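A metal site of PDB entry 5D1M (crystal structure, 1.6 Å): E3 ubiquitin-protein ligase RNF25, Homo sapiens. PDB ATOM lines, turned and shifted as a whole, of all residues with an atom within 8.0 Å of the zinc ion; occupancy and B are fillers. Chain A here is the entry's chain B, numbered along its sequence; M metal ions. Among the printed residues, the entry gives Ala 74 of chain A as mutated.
The backbone NH (N) of His 30 lies within hydrogen-bond range of the side-chain hydroxyl (OG1) of Thr 26.
The side-chain sulfur (SG) of Cys 73 sits close to the backbone NH (N) of Val 75 (3.4 Å).
The backbone NH (N) of Cys 73 is in hydrogen-bond range of the backbone carbonyl oxygen (O) of Glu 78 (2.8 Å).
The backbone NH of Cys 28 lies close to the side-chain hydroxyl of Thr 26.
Of the 16 residues printed, 4 come within 4 Å of the zinc ion.
The nearest printed residue that does not touch the zinc ion is Val 75 (4.3 Å).
The zinc ion is bound by a ring nitrogen (ND1) of His 30, the side-chain sulfur of Cys 73, the side-chain sulfur of Cys 28 and the side-chain sulfur of Cys 76.
The zinc ion has four donor atoms within binding distance.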
ATOM      1  N   THR A  26      -1.337 -27.688   5.807  1.00  0.00           N
ATOM      2  CA  THR A  26      -2.219 -26.635   5.253  1.00  0.00           C
ATOM      3  C   THR A  26      -3.319 -27.202   4.330  1.00  0.00           C
ATOM      4  O   THR A  26      -3.223 -28.356   3.900  1.00  0.00           O
ATOM      5  CB  THR A  26      -1.439 -25.587   4.406  1.00  0.00           C
ATOM      6  OG1 THR A  26      -0.894 -26.243   3.268  1.00  0.00           O
ATOM      7  CG2 THR A  26      -0.314 -24.919   5.201  1.00  0.00           C
ATOM      8  N   PRO A  27      -4.357 -26.404   4.000  1.00  0.00           N
ATOM      9  CA  PRO A  27      -5.384 -26.904   3.062  1.00  0.00           C
ATOM     10  C   PRO A  27      -4.856 -27.089   1.658  1.00  0.00           C
ATOM     11  O   PRO A  27      -5.533 -27.686   0.821  1.00  0.00           O
ATOM     12  CB  PRO A  27      -6.443 -25.794   3.056  1.00  0.00           C
ATOM     13  CG  PRO A  27      -6.232 -25.068   4.387  1.00  0.00           C
ATOM     14  CD  PRO A  27      -4.731 -25.085   4.557  1.00  0.00           C
ATOM     15  N   CYS A  28      -3.671 -26.564   1.391  1.00  0.00           N
ATOM     16  CA  CYS A  28      -2.978 -26.756   0.111  1.00  0.00           C
ATOM     17  C   CYS A  28      -1.935 -27.879   0.178  1.00  0.00           C
ATOM     18  O   CYS A  28      -1.099 -28.005  -0.727  1.00  0.00           O
ATOM     19  CB  CYS A  28      -2.390 -25.409  -0.390  1.00  0.00           C
ATOM     20  SG  CYS A  28      -1.351 -24.459   0.767  1.00  0.00           S
ATOM     21  N   TYR A  29      -2.003 -28.695   1.242  1.00  0.00           N
ATOM     22  CA  TYR A  29      -1.303 -29.998   1.348  1.00  0.00           C
ATOM     23  C   TYR A  29       0.179 -29.923   1.662  1.00  0.00           C
ATOM     24  O   TYR A  29       0.938 -30.844   1.378  1.00  0.00           O
ATOM     25  CB  TYR A  29      -1.544 -30.887   0.101  1.00  0.00           C
ATOM     26  CG  TYR A  29      -2.983 -30.905  -0.342  1.00  0.00           C
ATOM     27  CD1 TYR A  29      -3.968 -31.560   0.413  1.00  0.00           C
ATOM     28  CD2 TYR A  29      -3.377 -30.269  -1.511  1.00  0.00           C
ATOM     29  CE1 TYR A  29      -5.299 -31.562   0.024  1.00  0.00           C
ATOM     30  CE2 TYR A  29      -4.722 -30.258  -1.916  1.00  0.00           C
ATOM     31  CZ  TYR A  29      -5.672 -30.913  -1.146  1.00  0.00           C
ATOM     32  OH  TYR A  29      -6.988 -30.903  -1.558  1.00  0.00           O
ATOM     33  N   HIS A  30       0.568 -28.816   2.301  1.00  0.00           N
ATOM     34  CA  HIS A  30       1.965 -28.569   2.644  1.00  0.00           C
ATOM     35  C   HIS A  30       2.171 -28.665   4.157  1.00  0.00           C
ATOM     36  O   HIS A  30       1.375 -28.103   4.908  1.00  0.00           O
ATOM     37  CB  HIS A  30       2.367 -27.214   2.025  1.00  0.00           C
ATOM     38  CG  HIS A  30       2.363 -27.244   0.528  1.00  0.00           C
ATOM     39  ND1 HIS A  30       1.712 -26.308  -0.264  1.00  0.00           N
ATOM     40  CD2 HIS A  30       2.882 -28.147  -0.334  1.00  0.00           C
ATOM     41  CE1 HIS A  30       1.862 -26.624  -1.538  1.00  0.00           C
ATOM     42  NE2 HIS A  30       2.558 -27.742  -1.613  1.00  0.00           N
ATOM     43  N   TYR A  31       3.217 -29.376   4.577  1.00  0.00           N
ATOM     44  CA  TYR A  31       3.506 -29.615   6.007  1.00  0.00           C
ATOM     45  C   TYR A  31       4.596 -28.665   6.511  1.00  0.00           C
ATOM     46  O   TYR A  31       5.616 -28.446   5.838  1.00  0.00           O
ATOM     47  CB  TYR A  31       3.974 -31.076   6.254  1.00  0.00           C
ATOM     48  CG  TYR A  31       2.912 -32.164   6.089  1.00  0.00           C
ATOM     49  CD1 TYR A  31       2.643 -32.723   4.856  1.00  0.00           C
ATOM     50  CD2 TYR A  31       2.203 -32.630   7.191  1.00  0.00           C
ATOM     51  CE1 TYR A  31       1.678 -33.714   4.724  1.00  0.00           C
ATOM     52  CE2 TYR A  31       1.243 -33.611   7.077  1.00  0.00           C
ATOM     53  CZ  TYR A  31       0.983 -34.162   5.836  1.00  0.00           C
ATOM     54  OH  TYR A  31       0.020 -35.139   5.708  1.00  0.00           O
ATOM     55  N   PHE A  32       4.378 -28.123   7.706  1.00  0.00           N
ATOM     56  CA  PHE A  32       5.391 -27.288   8.385  1.00  0.00           C
ATOM     57  C   PHE A  32       5.398 -27.637   9.868  1.00  0.00           C
ATOM     58  O   PHE A  32       4.364 -28.027  10.407  1.00  0.00           O
ATOM     59  CB  PHE A  32       5.029 -25.794   8.220  1.00  0.00           C
ATOM     60  CG  PHE A  32       4.863 -25.332   6.776  1.00  0.00           C
ATOM     61  CD1 PHE A  32       5.951 -24.853   6.060  1.00  0.00           C
ATOM     62  CD2 PHE A  32       3.609 -25.339   6.163  1.00  0.00           C
ATOM     63  CE1 PHE A  32       5.804 -24.424   4.738  1.00  0.00           C
ATOM     64  CE2 PHE A  32       3.455 -24.904   4.852  1.00  0.00           C
ATOM     65  CZ  PHE A  32       4.551 -24.440   4.131  1.00  0.00           C
ATOM     66  N   GLN A  72       0.139 -15.392   2.208  1.00  0.00           N
ATOM     67  CA  GLN A  72       0.112 -16.511   1.252  1.00  0.00           C
ATOM     68  C   GLN A  72       1.037 -17.662   1.671  1.00  0.00           C
ATOM     69  O   GLN A  72       2.038 -17.438   2.373  1.00  0.00           O
ATOM     70  CB  GLN A  72       0.556 -15.995  -0.127  1.00  0.00           C
ATOM     71  CG  GLN A  72      -0.292 -14.864  -0.689  1.00  0.00           C
ATOM     72  CD  GLN A  72       0.365 -14.186  -1.880  1.00  0.00           C
ATOM     73  OE1 GLN A  72       1.577 -14.286  -2.092  1.00  0.00           O
ATOM     74  NE2 GLN A  72      -0.446 -13.486  -2.675  1.00  0.00           N
ATOM     75  N   CYS A  73       0.734 -18.888   1.233  1.00  0.00           N
ATOM     76  CA  CYS A  73       1.607 -20.052   1.495  1.00  0.00           C
ATOM     77  C   CYS A  73       3.005 -19.803   0.958  1.00  0.00           C
ATOM     78  O   CYS A  73       3.143 -19.350  -0.185  1.00  0.00           O
ATOM     79  CB  CYS A  73       1.034 -21.360   0.874  1.00  0.00           C
ATOM     80  SG  CYS A  73       2.036 -22.859   1.118  1.00  0.00           S
ATOM     81  N   ALA A  74       4.013 -20.092   1.773  1.00  0.00           N
ATOM     82  CA  ALA A  74       5.414 -19.930   1.347  1.00  0.00           C
ATOM     83  C   ALA A  74       5.737 -20.745   0.105  1.00  0.00           C
ATOM     84  O   ALA A  74       6.564 -20.339  -0.719  1.00  0.00           O
ATOM     85  CB  ALA A  74       6.351 -20.332   2.480  1.00  0.00           C
ATOM     86  N   VAL A  75       5.096 -21.897  -0.012  1.00  0.00           N
ATOM     87  CA  VAL A  75       5.368 -22.815  -1.105  1.00  0.00           C
ATOM     88  C   VAL A  75       4.633 -22.456  -2.403  1.00  0.00           C
ATOM     89  O   VAL A  75       5.256 -22.356  -3.466  1.00  0.00           O
ATOM     90  CB  VAL A  75       5.042 -24.278  -0.684  1.00  0.00           C
ATOM     91  CG1 VAL A  75       5.150 -25.246  -1.879  1.00  0.00           C
ATOM     92  CG2 VAL A  75       5.980 -24.740   0.425  1.00  0.00           C
ATOM     93  N   CYS A  76       3.315 -22.239  -2.314  1.00  0.00           N
ATOM     94  CA  CYS A  76       2.471 -22.143  -3.531  1.00  0.00           C
ATOM     95  C   CYS A  76       1.652 -20.858  -3.689  1.00  0.00           C
ATOM     96  O   CYS A  76       0.897 -20.702  -4.655  1.00  0.00           O
ATOM     97  CB  CYS A  76       1.521 -23.365  -3.624  1.00  0.00           C
ATOM     98  SG  CYS A  76       0.247 -23.402  -2.336  1.00  0.00           S
ATOM     99  N   ARG A  77       1.778 -19.932  -2.742  1.00  0.00           N
ATOM    100  CA  ARG A  77       1.084 -18.626  -2.745  1.00  0.00           C
ATOM    101  C   ARG A  77      -0.437 -18.639  -2.542  1.00  0.00           C
ATOM    102  O   ARG A  77      -1.063 -17.580  -2.621  1.00  0.00           O
ATOM    103  CB  ARG A  77       1.452 -17.777  -3.977  1.00  0.00           C
ATOM    104  CG  ARG A  77       2.929 -17.479  -4.098  1.00  0.00           C
ATOM    105  CD  ARG A  77       3.244 -16.535  -5.239  1.00  0.00           C
ATOM    106  NE  ARG A  77       4.693 -16.345  -5.322  1.00  0.00           N
ATOM    107  CZ  ARG A  77       5.372 -15.459  -4.587  1.00  0.00           C
ATOM    108  NH1 ARG A  77       4.751 -14.714  -3.684  1.00  0.00           N
ATOM    109  NH2 ARG A  77       6.679 -15.315  -4.770  1.00  0.00           N
ATOM    110  N   GLU A  78      -1.029 -19.813  -2.264  1.00  0.00           N
ATOM    111  CA  GLU A  78      -2.435 -19.845  -1.891  1.00  0.00           C
ATOM    112  C   GLU A  78      -2.630 -19.093  -0.577  1.00  0.00           C
ATOM    113  O   GLU A  78      -1.850 -19.260   0.365  1.00  0.00           O
ATOM    114  CB  GLU A  78      -2.966 -21.279  -1.751  1.00  0.00           C
ATOM    115  CG  GLU A  78      -4.384 -21.366  -1.172  1.00  0.00           C
ATOM    116  CD  GLU A  78      -5.007 -22.755  -1.322  1.00  0.00           C
ATOM    117  OE1 GLU A  78      -4.909 -23.329  -2.414  1.00  0.00           O
ATOM    118  OE2 GLU A  78      -5.619 -23.258  -0.358  1.00  0.00           O
ATOM    119  N   PRO A  79      -3.676 -18.260  -0.504  1.00  0.00           N
ATOM    120  CA  PRO A  79      -3.893 -17.586   0.779  1.00  0.00           C
ATOM    121  C   PRO A  79      -4.178 -18.579   1.929  1.00  0.00           C
ATOM    122  O   PRO A  79      -5.021 -19.474   1.765  1.00  0.00           O
ATOM    123  CB  PRO A  79      -5.114 -16.715   0.483  1.00  0.00           C
ATOM    124  CG  PRO A  79      -5.045 -16.463  -1.000  1.00  0.00           C
ATOM    125  CD  PRO A  79      -4.548 -17.766  -1.567  1.00  0.00           C
ATOM    126  N   LEU A  80      -3.496 -18.428   3.057  1.00  0.00           N
ATOM    127  CA  LEU A  80      -3.661 -19.370   4.177  1.00  0.00           C
ATOM    128  C   LEU A  80      -4.809 -19.027   5.103  1.00  0.00           C
ATOM    129  O   LEU A  80      -5.141 -17.848   5.251  1.00  0.00           O
ATOM    130  CB  LEU A  80      -2.389 -19.446   5.003  1.00  0.00           C
ATOM    131  CG  LEU A  80      -1.114 -20.028   4.388  1.00  0.00           C
ATOM    132  CD1 LEU A  80      -0.040 -20.030   5.432  1.00  0.00           C
ATOM    133  CD2 LEU A  80      -1.380 -21.430   3.901  1.00  0.00           C
HETATM  134 ZN    ZN M   1       0.793 -24.336  -0.179  1.00  0.00          ZN
